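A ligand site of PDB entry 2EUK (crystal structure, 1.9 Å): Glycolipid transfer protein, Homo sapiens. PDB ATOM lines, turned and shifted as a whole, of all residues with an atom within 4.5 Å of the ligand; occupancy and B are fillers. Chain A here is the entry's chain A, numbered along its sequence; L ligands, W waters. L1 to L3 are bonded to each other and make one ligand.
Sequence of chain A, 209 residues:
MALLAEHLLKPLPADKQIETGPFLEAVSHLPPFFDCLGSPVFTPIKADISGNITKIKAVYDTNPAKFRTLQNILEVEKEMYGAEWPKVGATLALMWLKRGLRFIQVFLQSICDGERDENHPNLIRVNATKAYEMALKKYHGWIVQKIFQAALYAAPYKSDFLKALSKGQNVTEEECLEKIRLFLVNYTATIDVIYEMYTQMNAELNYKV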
ATOM      1  N   LEU A  30      20.341  17.678   8.322  1.00  0.00           N
ATOM      2  CA  LEU A  30      21.043  16.537   8.918  1.00  0.00           C
ATOM      3  C   LEU A  30      20.875  16.365  10.435  1.00  0.00           C
ATOM      4  O   LEU A  30      20.629  15.239  10.861  1.00  0.00           O
ATOM      5  CB  LEU A  30      22.504  16.412   8.459  1.00  0.00           C
ATOM      6  CG  LEU A  30      22.728  16.358   6.939  1.00  0.00           C
ATOM      7  CD1 LEU A  30      24.196  16.603   6.638  1.00  0.00           C
ATOM      8  CD2 LEU A  30      22.328  14.996   6.376  1.00  0.00           C
ATOM      9  N   PHE A  33      18.188  14.003  11.892  1.00  0.00           N
ATOM     10  CA  PHE A  33      18.364  12.552  11.858  1.00  0.00           C
ATOM     11  C   PHE A  33      18.821  11.975  13.202  1.00  0.00           C
ATOM     12  O   PHE A  33      18.554  10.816  13.496  1.00  0.00           O
ATOM     13  CB  PHE A  33      19.353  12.125  10.763  1.00  0.00           C
ATOM     14  CG  PHE A  33      18.783  12.190   9.377  1.00  0.00           C
ATOM     15  CD1 PHE A  33      18.794  13.386   8.657  1.00  0.00           C
ATOM     16  CD2 PHE A  33      18.213  11.070   8.791  1.00  0.00           C
ATOM     17  CE1 PHE A  33      18.256  13.460   7.382  1.00  0.00           C
ATOM     18  CE2 PHE A  33      17.682  11.118   7.501  1.00  0.00           C
ATOM     19  CZ  PHE A  33      17.703  12.311   6.790  1.00  0.00           C
ATOM     20  N   PHE A  34      19.504  12.804  13.993  1.00  0.00           N
ATOM     21  CA  PHE A  34      19.998  12.433  15.323  1.00  0.00           C
ATOM     22  C   PHE A  34      18.913  12.223  16.377  1.00  0.00           C
ATOM     23  O   PHE A  34      19.160  11.557  17.387  1.00  0.00           O
ATOM     24  CB  PHE A  34      21.044  13.428  15.822  1.00  0.00           C
ATOM     25  CG  PHE A  34      22.377  13.294  15.144  1.00  0.00           C
ATOM     26  CD1 PHE A  34      23.245  12.273  15.508  1.00  0.00           C
ATOM     27  CD2 PHE A  34      22.746  14.154  14.132  1.00  0.00           C
ATOM     28  CE1 PHE A  34      24.470  12.121  14.880  1.00  0.00           C
ATOM     29  CE2 PHE A  34      23.971  14.012  13.493  1.00  0.00           C
ATOM     30  CZ  PHE A  34      24.839  13.008  13.874  1.00  0.00           C
ATOM     31  N   LEU A  37      17.730   8.227  16.250  1.00  0.00           N
ATOM     32  CA  LEU A  37      18.685   7.141  16.514  1.00  0.00           C
ATOM     33  C   LEU A  37      18.431   6.427  17.844  1.00  0.00           C
ATOM     34  O   LEU A  37      19.164   5.502  18.209  1.00  0.00           O
ATOM     35  CB  LEU A  37      20.114   7.676  16.486  1.00  0.00           C
ATOM     36  CG  LEU A  37      20.898   7.673  15.165  1.00  0.00           C
ATOM     37  CD1 LEU A  37      19.996   7.917  13.963  1.00  0.00           C
ATOM     38  CD2 LEU A  37      22.002   8.694  15.224  1.00  0.00           C
ATOM     39  N   PHE A  42      22.668  11.217  21.771  1.00  0.00           N
ATOM     40  CA  PHE A  42      22.812  12.053  20.574  1.00  0.00           C
ATOM     41  C   PHE A  42      22.451  13.521  20.761  1.00  0.00           C
ATOM     42  O   PHE A  42      22.699  14.313  19.857  1.00  0.00           O
ATOM     43  CB  PHE A  42      22.039  11.449  19.409  1.00  0.00           C
ATOM     44  CG  PHE A  42      22.528  10.090  19.036  1.00  0.00           C
ATOM     45  CD1 PHE A  42      23.758   9.930  18.410  1.00  0.00           C
ATOM     46  CD2 PHE A  42      21.805   8.965  19.401  1.00  0.00           C
ATOM     47  CE1 PHE A  42      24.228   8.653  18.092  1.00  0.00           C
ATOM     48  CE2 PHE A  42      22.269   7.686  19.091  1.00  0.00           C
ATOM     49  CZ  PHE A  42      23.472   7.539  18.445  1.00  0.00           C
ATOM     50  N   PRO A  44      23.729  16.061  22.697  1.00  0.00           N
ATOM     51  CA  PRO A  44      24.810  17.060  22.584  1.00  0.00           C
ATOM     52  C   PRO A  44      25.527  17.064  21.234  1.00  0.00           C
ATOM     53  O   PRO A  44      26.203  18.026  20.884  1.00  0.00           O
ATOM     54  CB  PRO A  44      25.807  16.643  23.680  1.00  0.00           C
ATOM     55  CG  PRO A  44      25.126  15.608  24.450  1.00  0.00           C
ATOM     56  CD  PRO A  44      24.113  14.952  23.602  1.00  0.00           C
ATOM     57  N   ILE A  45      25.436  15.944  20.524  1.00  0.00           N
ATOM     58  CA  ILE A  45      26.026  15.818  19.181  1.00  0.00           C
ATOM     59  C   ILE A  45      25.246  16.690  18.202  1.00  0.00           C
ATOM     60  O   ILE A  45      25.801  17.516  17.463  1.00  0.00           O
ATOM     61  CB  ILE A  45      25.999  14.340  18.765  1.00  0.00           C
ATOM     62  CG1 ILE A  45      27.097  13.572  19.506  1.00  0.00           C
ATOM     63  CG2 ILE A  45      26.120  14.211  17.260  1.00  0.00           C
ATOM     64  CD1 ILE A  45      26.937  12.062  19.437  1.00  0.00           C
ATOM     65  N   ASP A  48      26.002  20.381  18.923  1.00  0.00           N
ATOM     66  CA  ASP A  48      27.279  20.828  18.343  1.00  0.00           C
ATOM     67  C   ASP A  48      27.143  21.199  16.866  1.00  0.00           C
ATOM     68  O   ASP A  48      27.575  22.281  16.428  1.00  0.00           O
ATOM     69  CB  ASP A  48      28.401  19.787  18.560  1.00  0.00           C
ATOM     70  CG  ASP A  48      29.760  20.310  18.081  1.00  0.00           C
ATOM     71  OD1 ASP A  48      30.526  20.909  18.878  1.00  0.00           O
ATOM     72  OD2 ASP A  48      30.039  20.209  16.866  1.00  0.00           O
ATOM     73  N   ILE A  49      26.553  20.271  16.118  1.00  0.00           N
ATOM     74  CA  ILE A  49      26.482  20.394  14.667  1.00  0.00           C
ATOM     75  C   ILE A  49      25.524  21.566  14.407  1.00  0.00           C
ATOM     76  O   ILE A  49      25.856  22.501  13.688  1.00  0.00           O
ATOM     77  CB  ILE A  49      25.996  19.090  13.963  1.00  0.00           C
ATOM     78  CG1 ILE A  49      27.034  17.949  14.085  1.00  0.00           C
ATOM     79  CG2 ILE A  49      25.744  19.447  12.490  1.00  0.00           C
ATOM     80  CD1 ILE A  49      26.575  16.535  13.741  1.00  0.00           C
ATOM     81  N   ASN A  52      27.062  25.017  15.250  1.00  0.00           N
ATOM     82  CA  ASN A  52      27.953  25.558  14.226  1.00  0.00           C
ATOM     83  C   ASN A  52      27.254  26.075  12.994  1.00  0.00           C
ATOM     84  O   ASN A  52      27.602  27.131  12.492  1.00  0.00           O
ATOM     85  CB  ASN A  52      28.992  24.515  13.862  1.00  0.00           C
ATOM     86  CG  ASN A  52      30.041  24.387  14.936  1.00  0.00           C
ATOM     87  OD1 ASN A  52      30.559  25.374  15.447  1.00  0.00           O
ATOM     88  ND2 ASN A  52      30.399  23.146  15.280  1.00  0.00           N
ATOM     89  N   LYS A  55      25.991  29.434  14.058  1.00  0.00           N
ATOM     90  CA  LYS A  55      27.097  30.387  14.130  1.00  0.00           C
ATOM     91  C   LYS A  55      27.419  30.926  12.737  1.00  0.00           C
ATOM     92  O   LYS A  55      27.662  32.132  12.553  1.00  0.00           O
ATOM     93  CB  LYS A  55      28.351  29.772  14.799  1.00  0.00           C
ATOM     94  CG  LYS A  55      28.217  29.617  16.335  1.00  0.00           C
ATOM     95  CD  LYS A  55      29.484  29.109  17.040  1.00  0.00           C
ATOM     96  CE  LYS A  55      29.160  28.592  18.463  1.00  0.00           C
ATOM     97  NZ  LYS A  55      30.348  27.891  19.043  1.00  0.00           N
ATOM     98  N   LEU A  92      35.905  29.456  12.453  1.00  0.00           N
ATOM     99  CA  LEU A  92      36.040  28.460  13.479  1.00  0.00           C
ATOM    100  C   LEU A  92      34.885  27.484  13.506  1.00  0.00           C
ATOM    101  O   LEU A  92      35.106  26.269  13.605  1.00  0.00           O
ATOM    102  CB  LEU A  92      36.251  29.046  14.878  1.00  0.00           C
ATOM    103  CG  LEU A  92      36.589  27.986  15.944  1.00  0.00           C
ATOM    104  CD1 LEU A  92      37.849  27.112  15.648  1.00  0.00           C
ATOM    105  CD2 LEU A  92      36.711  28.836  17.193  1.00  0.00           C
ATOM    106  N   TRP A  96      34.902  23.217  12.554  1.00  0.00           N
ATOM    107  CA  TRP A  96      34.324  22.091  13.298  1.00  0.00           C
ATOM    108  C   TRP A  96      33.107  21.484  12.622  1.00  0.00           C
ATOM    109  O   TRP A  96      32.879  20.258  12.680  1.00  0.00           O
ATOM    110  CB  TRP A  96      33.994  22.555  14.728  1.00  0.00           C
ATOM    111  CG  TRP A  96      35.238  22.708  15.591  1.00  0.00           C
ATOM    112  CD1 TRP A  96      35.975  23.842  15.816  1.00  0.00           C
ATOM    113  CD2 TRP A  96      35.965  21.633  16.184  1.00  0.00           C
ATOM    114  NE1 TRP A  96      37.073  23.527  16.608  1.00  0.00           N
ATOM    115  CE2 TRP A  96      37.069  22.182  16.870  1.00  0.00           C
ATOM    116  CE3 TRP A  96      35.741  20.242  16.261  1.00  0.00           C
ATOM    117  CZ2 TRP A  96      37.975  21.397  17.604  1.00  0.00           C
ATOM    118  CZ3 TRP A  96      36.585  19.479  16.999  1.00  0.00           C
ATOM    119  CH2 TRP A  96      37.713  20.052  17.672  1.00  0.00           C
ATOM    120  N   GLY A 100      32.306  17.396  11.623  1.00  0.00           N
ATOM    121  CA  GLY A 100      31.062  16.641  11.853  1.00  0.00           C
ATOM    122  C   GLY A 100      30.446  16.105  10.545  1.00  0.00           C
ATOM    123  O   GLY A 100      29.982  14.952  10.470  1.00  0.00           O
ATOM    124  N   PHE A 103      32.584  13.239   9.342  1.00  0.00           N
ATOM    125  CA  PHE A 103      32.177  12.056  10.099  1.00  0.00           C
ATOM    126  C   PHE A 103      30.964  11.361   9.486  1.00  0.00           C
ATOM    127  O   PHE A 103      30.977  10.126   9.267  1.00  0.00           O
ATOM    128  CB  PHE A 103      31.939  12.333  11.605  1.00  0.00           C
ATOM    129  CG  PHE A 103      31.406  11.117  12.327  1.00  0.00           C
ATOM    130  CD1 PHE A 103      32.257  10.336  13.107  1.00  0.00           C
ATOM    131  CD2 PHE A 103      30.056  10.738  12.217  1.00  0.00           C
ATOM    132  CE1 PHE A 103      31.760   9.186  13.767  1.00  0.00           C
ATOM    133  CE2 PHE A 103      29.555   9.592  12.861  1.00  0.00           C
ATOM    134  CZ  PHE A 103      30.407   8.820  13.631  1.00  0.00           C
ATOM    135  N   ILE A 104      29.894  12.104   9.205  1.00  0.00           N
ATOM    136  CA  ILE A 104      28.683  11.518   8.619  1.00  0.00           C
ATOM    137  C   ILE A 104      28.985  10.894   7.249  1.00  0.00           C
ATOM    138  O   ILE A 104      28.519   9.786   6.902  1.00  0.00           O
ATOM    139  CB  ILE A 104      27.529  12.553   8.520  1.00  0.00           C
ATOM    140  CG1 ILE A 104      27.142  13.000   9.936  1.00  0.00           C
ATOM    141  CG2 ILE A 104      26.271  11.993   7.805  1.00  0.00           C
ATOM    142  CD1 ILE A 104      26.423  14.268  10.011  1.00  0.00           C
ATOM    143  N   PHE A 107      31.142   7.567   7.630  1.00  0.00           N
ATOM    144  CA  PHE A 107      30.239   6.569   8.205  1.00  0.00           C
ATOM    145  C   PHE A 107      29.246   6.043   7.150  1.00  0.00           C
ATOM    146  O   PHE A 107      29.149   4.824   6.934  1.00  0.00           O
ATOM    147  CB  PHE A 107      29.437   7.226   9.325  1.00  0.00           C
ATOM    148  CG  PHE A 107      28.395   6.354   9.957  1.00  0.00           C
ATOM    149  CD1 PHE A 107      28.757   5.338  10.811  1.00  0.00           C
ATOM    150  CD2 PHE A 107      27.035   6.623   9.759  1.00  0.00           C
ATOM    151  CE1 PHE A 107      27.798   4.540  11.463  1.00  0.00           C
ATOM    152  CE2 PHE A 107      26.054   5.848  10.411  1.00  0.00           C
ATOM    153  CZ  PHE A 107      26.440   4.801  11.239  1.00  0.00           C
ATOM    154  N   ILE A 124      27.020  -1.550  13.707  1.00  0.00           N
ATOM    155  CA  ILE A 124      27.595  -0.469  12.909  1.00  0.00           C
ATOM    156  C   ILE A 124      28.763   0.184  13.635  1.00  0.00           C
ATOM    157  O   ILE A 124      29.165   1.307  13.301  1.00  0.00           O
ATOM    158  CB  ILE A 124      26.588   0.632  12.497  1.00  0.00           C
ATOM    159  CG1 ILE A 124      25.978   1.284  13.743  1.00  0.00           C
ATOM    160  CG2 ILE A 124      25.545   0.087  11.556  1.00  0.00           C
ATOM    161  CD1 ILE A 124      24.998   2.379  13.445  1.00  0.00           C
ATOM    162  N   ALA A 128      31.274   3.296  12.492  1.00  0.00           N
ATOM    163  CA  ALA A 128      31.355   4.517  13.298  1.00  0.00           C
ATOM    164  C   ALA A 128      32.784   4.794  13.760  1.00  0.00           C
ATOM    165  O   ALA A 128      33.297   5.929  13.725  1.00  0.00           O
ATOM    166  CB  ALA A 128      30.403   4.371  14.467  1.00  0.00           C
ATOM    167  N   LEU A 136      37.436  12.840  13.395  1.00  0.00           N
ATOM    168  CA  LEU A 136      37.341  13.542  14.667  1.00  0.00           C
ATOM    169  C   LEU A 136      38.505  13.274  15.619  1.00  0.00           C
ATOM    170  O   LEU A 136      38.964  14.211  16.282  1.00  0.00           O
ATOM    171  CB  LEU A 136      36.031  13.258  15.388  1.00  0.00           C
ATOM    172  CG  LEU A 136      34.821  13.902  14.684  1.00  0.00           C
ATOM    173  CD1 LEU A 136      33.509  13.311  15.201  1.00  0.00           C
ATOM    174  CD2 LEU A 136      34.865  15.410  14.827  1.00  0.00           C
ATOM    175  N   HIS A 140      40.550  15.349  19.433  1.00  0.00           N
ATOM    176  CA  HIS A 140      40.067  15.045  20.768  1.00  0.00           C
ATOM    177  C   HIS A 140      41.183  14.569  21.712  1.00  0.00           C
ATOM    178  O   HIS A 140      41.964  13.663  21.373  1.00  0.00           O
ATOM    179  CB  HIS A 140      38.967  13.978  20.715  1.00  0.00           C
ATOM    180  CG  HIS A 140      37.727  14.428  20.007  1.00  0.00           C
ATOM    181  ND1 HIS A 140      36.686  13.574  19.732  1.00  0.00           N
ATOM    182  CD2 HIS A 140      37.358  15.655  19.570  1.00  0.00           C
ATOM    183  CE1 HIS A 140      35.720  14.263  19.127  1.00  0.00           C
ATOM    184  NE2 HIS A 140      36.103  15.527  19.024  1.00  0.00           N
ATOM    185  N   ILE A 147      34.751   9.173  26.108  1.00  0.00           N
ATOM    186  CA  ILE A 147      33.311   9.389  25.950  1.00  0.00           C
ATOM    187  C   ILE A 147      32.778   8.837  24.615  1.00  0.00           C
ATOM    188  O   ILE A 147      31.726   8.180  24.577  1.00  0.00           O
ATOM    189  CB  ILE A 147      32.942  10.891  26.178  1.00  0.00           C
ATOM    190  CG1 ILE A 147      33.321  11.267  27.621  1.00  0.00           C
ATOM    191  CG2 ILE A 147      31.442  11.129  25.907  1.00  0.00           C
ATOM    192  CD1 ILE A 147      33.508  12.734  27.918  1.00  0.00           C
ATOM    193  N   PHE A 148      33.529   9.067  23.533  1.00  0.00           N
ATOM    194  CA  PHE A 148      33.167   8.414  22.269  1.00  0.00           C
ATOM    195  C   PHE A 148      33.078   6.883  22.403  1.00  0.00           C
ATOM    196  O   PHE A 148      32.129   6.235  21.934  1.00  0.00           O
ATOM    197  CB  PHE A 148      34.103   8.804  21.115  1.00  0.00           C
ATOM    198  CG  PHE A 148      33.869   7.940  19.899  1.00  0.00           C
ATOM    199  CD1 PHE A 148      32.814   8.212  19.041  1.00  0.00           C
ATOM    200  CD2 PHE A 148      34.626   6.786  19.682  1.00  0.00           C
ATOM    201  CE1 PHE A 148      32.554   7.399  17.949  1.00  0.00           C
ATOM    202  CE2 PHE A 148      34.395   5.980  18.590  1.00  0.00           C
ATOM    203  CZ  PHE A 148      33.335   6.273  17.733  1.00  0.00           C
ATOM    204  N   ALA A 151      29.847   6.128  24.084  1.00  0.00           N
ATOM    205  CA  ALA A 151      28.693   6.504  23.285  1.00  0.00           C
ATOM    206  C   ALA A 151      28.517   5.495  22.152  1.00  0.00           C
ATOM    207  O   ALA A 151      27.403   5.274  21.679  1.00  0.00           O
ATOM    208  CB  ALA A 151      28.876   7.931  22.766  1.00  0.00           C
ATOM    209  N   LEU A 152      29.609   4.866  21.729  1.00  0.00           N
ATOM    210  CA  LEU A 152      29.574   3.870  20.653  1.00  0.00           C
ATOM    211  C   LEU A 152      28.537   2.802  20.989  1.00  0.00           C
ATOM    212  O   LEU A 152      27.872   2.278  20.110  1.00  0.00           O
ATOM    213  CB  LEU A 152      30.970   3.264  20.443  1.00  0.00           C
ATOM    214  CG  LEU A 152      31.268   2.377  19.224  1.00  0.00           C
ATOM    215  CD1 LEU A 152      30.799   3.024  17.925  1.00  0.00           C
ATOM    216  CD2 LEU A 152      32.766   2.101  19.204  1.00  0.00           C
ATOM    217  N   ALA A 155      24.872   3.073  19.547  1.00  0.00           N
ATOM    218  CA  ALA A 155      24.583   2.814  18.128  1.00  0.00           C
ATOM    219  C   ALA A 155      23.422   1.825  17.907  1.00  0.00           C
ATOM    220  O   ALA A 155      23.386   0.782  18.573  1.00  0.00           O
ATOM    221  CB  ALA A 155      25.807   2.307  17.404  1.00  0.00           C
ATOM    222  N   PHE A 161      19.033   0.975  11.903  1.00  0.00           N
ATOM    223  CA  PHE A 161      19.501   2.252  11.381  1.00  0.00           C
ATOM    224  C   PHE A 161      18.892   2.570  10.007  1.00  0.00           C
ATOM    225  O   PHE A 161      18.436   3.689   9.751  1.00  0.00           O
ATOM    226  CB  PHE A 161      21.032   2.275  11.297  1.00  0.00           C
ATOM    227  CG  PHE A 161      21.589   3.551  10.744  1.00  0.00           C
ATOM    228  CD1 PHE A 161      21.434   4.743  11.446  1.00  0.00           C
ATOM    229  CD2 PHE A 161      22.277   3.563   9.544  1.00  0.00           C
ATOM    230  CE1 PHE A 161      21.955   5.940  10.951  1.00  0.00           C
ATOM    231  CE2 PHE A 161      22.788   4.744   9.023  1.00  0.00           C
ATOM    232  CZ  PHE A 161      22.632   5.941   9.739  1.00  0.00           C
ATOM    233  N   TYR A 207      44.530  21.961  17.238  1.00  0.00           N
ATOM    234  CA  TYR A 207      44.337  21.869  18.670  1.00  0.00           C
ATOM    235  C   TYR A 207      43.301  20.794  19.059  1.00  0.00           C
ATOM    236  O   TYR A 207      42.346  20.549  18.316  1.00  0.00           O
ATOM    237  CB  TYR A 207      43.983  23.253  19.259  1.00  0.00           C
ATOM    238  CG  TYR A 207      42.543  23.705  19.062  1.00  0.00           C
ATOM    239  CD1 TYR A 207      41.535  23.339  19.945  1.00  0.00           C
ATOM    240  CD2 TYR A 207      42.186  24.504  17.961  1.00  0.00           C
ATOM    241  CE1 TYR A 207      40.215  23.777  19.767  1.00  0.00           C
ATOM    242  CE2 TYR A 207      40.871  24.917  17.769  1.00  0.00           C
ATOM    243  CZ  TYR A 207      39.893  24.544  18.649  1.00  0.00           C
ATOM    244  OH  TYR A 207      38.591  25.001  18.452  1.00  0.00           O
ATOM    245  N   VAL A 209      40.533  19.048  21.874  1.00  0.00           N
ATOM    246  CA  VAL A 209      39.622  19.462  22.926  1.00  0.00           C
ATOM    247  C   VAL A 209      39.477  18.453  24.055  1.00  0.00           C
ATOM    248  O   VAL A 209      39.555  17.219  23.972  1.00  0.00           O
ATOM    249  CB  VAL A 209      38.230  19.866  22.383  1.00  0.00           C
ATOM    250  CG1 VAL A 209      38.324  21.188  21.617  1.00  0.00           C
ATOM    251  CG2 VAL A 209      37.608  18.788  21.508  1.00  0.00           C
ATOM    252  OXT VAL A 209      39.339  18.915  25.180  1.00  0.00           O
HETATM  253  C1  LIG L   1      33.783  23.021  19.031  1.00  0.00           C
HETATM  254  C2  LIG L   1      32.505  23.730  18.576  1.00  0.00           C
HETATM  255  C3  LIG L   1      32.837  25.106  17.986  1.00  0.00           C
HETATM  256  C4  LIG L   1      33.708  25.918  18.949  1.00  0.00           C
HETATM  257  C5  LIG L   1      34.910  25.069  19.358  1.00  0.00           C
HETATM  258  C6  LIG L   1      35.837  25.820  20.328  1.00  0.00           C
HETATM  259  O1  LIG L   1      33.492  21.793  19.609  1.00  0.00           O
HETATM  260  O2  LIG L   1      31.914  22.872  17.630  1.00  0.00           O
HETATM  261  O3  LIG L   1      31.654  25.835  17.739  1.00  0.00           O
HETATM  262  O4  LIG L   1      32.891  26.297  20.047  1.00  0.00           O
HETATM  263  O5  LIG L   1      34.544  23.824  19.922  1.00  0.00           O
HETATM  264  O6  LIG L   1      37.053  25.107  20.447  1.00  0.00           O
HETATM  265  C1  LG2 L   2      34.459  20.859  19.785  1.00  0.00           C
HETATM  266  C2  LG2 L   2      33.821  19.467  19.894  1.00  0.00           C
HETATM  267  N1  LG2 L   2      33.147  19.289  18.617  1.00  0.00           N
HETATM  268  C3  LG2 L   2      32.922  19.291  21.128  1.00  0.00           C
HETATM  269  O1  LG2 L   2      33.710  19.669  22.294  1.00  0.00           O
HETATM  270  C4  LG2 L   2      32.198  17.930  21.238  1.00  0.00           C
HETATM  271  C5  LG2 L   2      30.878  17.703  21.189  1.00  0.00           C
HETATM  272  C6  LG2 L   2      30.120  16.467  21.739  1.00  0.00           C
HETATM  273  C7  LG2 L   2      29.845  16.376  23.262  1.00  0.00           C
HETATM  274  C8  LG2 L   2      30.944  15.720  24.110  1.00  0.00           C
HETATM  275  C9  LG2 L   2      31.114  16.041  25.615  1.00  0.00           C
HETATM  276  C10 LG2 L   2      30.436  15.113  26.626  1.00  0.00           C
HETATM  277  C11 LG2 L   2      30.423  15.572  28.085  1.00  0.00           C
HETATM  278  C12 LG2 L   2      29.210  15.029  28.845  1.00  0.00           C
HETATM  279  C13 LG2 L   2      29.518  14.813  30.332  1.00  0.00           C
HETATM  280  C14 LG2 L   2      28.263  14.347  31.074  1.00  0.00           C
HETATM  281  C15 LG2 L   2      28.572  13.785  32.456  1.00  0.00           C
HETATM  282  C16 LG2 L   2      27.607  12.675  32.897  1.00  0.00           C
HETATM  283  C17 LG2 L   2      26.242  13.148  33.385  1.00  0.00           C
HETATM  284  C18 LG2 L   2      26.290  13.626  34.821  1.00  0.00           C
HETATM  285  O1  LG3 L   3      34.087  17.343  18.055  1.00  0.00           O
HETATM  286  C1  LG3 L   3      33.164  18.392  17.730  1.00  0.00           C
HETATM  287  C2  LG3 L   3      32.335  17.941  16.539  1.00  0.00           C
HETATM  288  C3  LG3 L   3      31.327  16.877  16.941  1.00  0.00           C
HETATM  289  C4  LG3 L   3      30.763  16.326  15.634  1.00  0.00           C
HETATM  290  C5  LG3 L   3      30.080  14.985  15.836  1.00  0.00           C
HETATM  291  C6  LG3 L   3      29.763  14.313  14.499  1.00  0.00           C
HETATM  292  C7  LG3 L   3      28.846  13.124  14.722  1.00  0.00           C
HETATM  293  C8  LG3 L   3      29.481  12.230  15.773  1.00  0.00           C
HETATM  294  C9  LG3 L   3      28.559  11.065  16.078  1.00  0.00           C
HETATM  295  C10 LG3 L   3      29.278  10.146  17.074  1.00  0.00           C
HETATM  296  C11 LG3 L   3      28.307   9.148  17.711  1.00  0.00           C
HETATM  297  C12 LG3 L   3      28.978   7.780  17.840  1.00  0.00           C
HETATM  298  C13 LG3 L   3      28.097   6.724  18.499  1.00  0.00           C
HETATM  299  C14 LG3 L   3      26.949   6.189  17.643  1.00  0.00           C
HETATM  300  C15 LG3 L   3      27.416   5.514  16.351  1.00  0.00           C
HETATM  301  C16 LG3 L   3      26.882   5.633  15.129  1.00  0.00           C
HETATM  302  C17 LG3 L   3      25.689   6.476  14.685  1.00  0.00           C
HETATM  303  C18 LG3 L   3      26.130   7.464  13.618  1.00  0.00           C
HETATM  304  C19 LG3 L   3      24.950   8.246  13.038  1.00  0.00           C
HETATM  305  C20 LG3 L   3      25.391   9.565  12.435  1.00  0.00           C
HETATM  306  C21 LG3 L   3      24.691   9.809  11.099  1.00  0.00           C
HETATM  307  C22 LG3 L   3      23.531  10.796  11.198  1.00  0.00           C
HETATM  308  C23 LG3 L   3      22.730  10.749   9.896  1.00  0.00           C
HETATM  309  C24 LG3 L   3      22.870  12.036   9.121  1.00  0.00           C
HETATM  310  O   HOH W   1      31.642  24.453  21.963  1.00  0.00           O
HETATM  311  O   HOH W   2      34.236  22.182  22.815  1.00  0.00           O
HETATM  312  O   HOH W   3      34.132  28.670  20.707  1.00  0.00           O
HETATM  313  O   HOH W   4      31.975  19.330  24.459  1.00  0.00           O
HETATM  314  O   HOH W   5      28.734  24.134  18.144  1.00  0.00           O
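Residues that only touch the ligand: Phe 33, Phe 34, Leu 37, Phe 42, Ile 45, Ile 49, Trp 96, Gly 100, Phe 103, Ile 104, Phe 107, Ala 128, Leu 136, Phe 148, Ala 151, Leu 152 and Ala 155.
Hydrophobic or aromatic side chains that line the ligand: Phe 33, Phe 34, Leu 37, Phe 42, Ile 45, Ile 49, Trp 96, Phe 103, Ile 104, Phe 107, Ala 128, Leu 136, His 140, Phe 148, Ala 155 and Tyr 207.
22 residues have an atom within 4 Å of the ligand: Phe 33, Phe 34, Leu 37, Phe 42, Ile 45, Asp 48, Ile 49, Asn 52, Lys 55, Trp 96, Gly 100, Phe 103, Ile 104, Phe 107, Ala 128, Leu 136, His 140, Phe 148, Ala 151, Leu 152, Ala 155 and Tyr 207.
The side-chain hydroxyl of Tyr 207 is in hydrogen-bond range of an oxygen (O6) of LIG L1, 2.5 Å away.
O3 of LIG L1 sits at hydrogen-bond distance from OD1 of Asn 52 (2.6 Å).
O2 of LIG L1 lies within hydrogen-bond range of OD1 of Asp 48, 2.7 Å away.
An oxygen (O3) of LIG L1 is in hydrogen-bond range of the side-chain amino group (NZ) of Lys 55, 2.8 Å away.
NE2 of His 140 is in hydrogen-bond range of O1 of LG3 L3 (2.9 Å).
Water W5 lies within hydrogen-bond range of the backbone carbonyl oxygen of Asp 48 (2.8 Å), an oxygen (O3) of LIG L1 (3.4 Å) and the backbone NH of Asn 52 (3.5 Å).
The indole nitrogen (NE1) of Trp 96 sits at hydrogen-bond distance from the side-chain hydroxyl (OH) of Tyr 207 (2.8 Å).
O of Asp 48 lies within hydrogen-bond range of ND2 of Asn 52 (3.2 Å).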
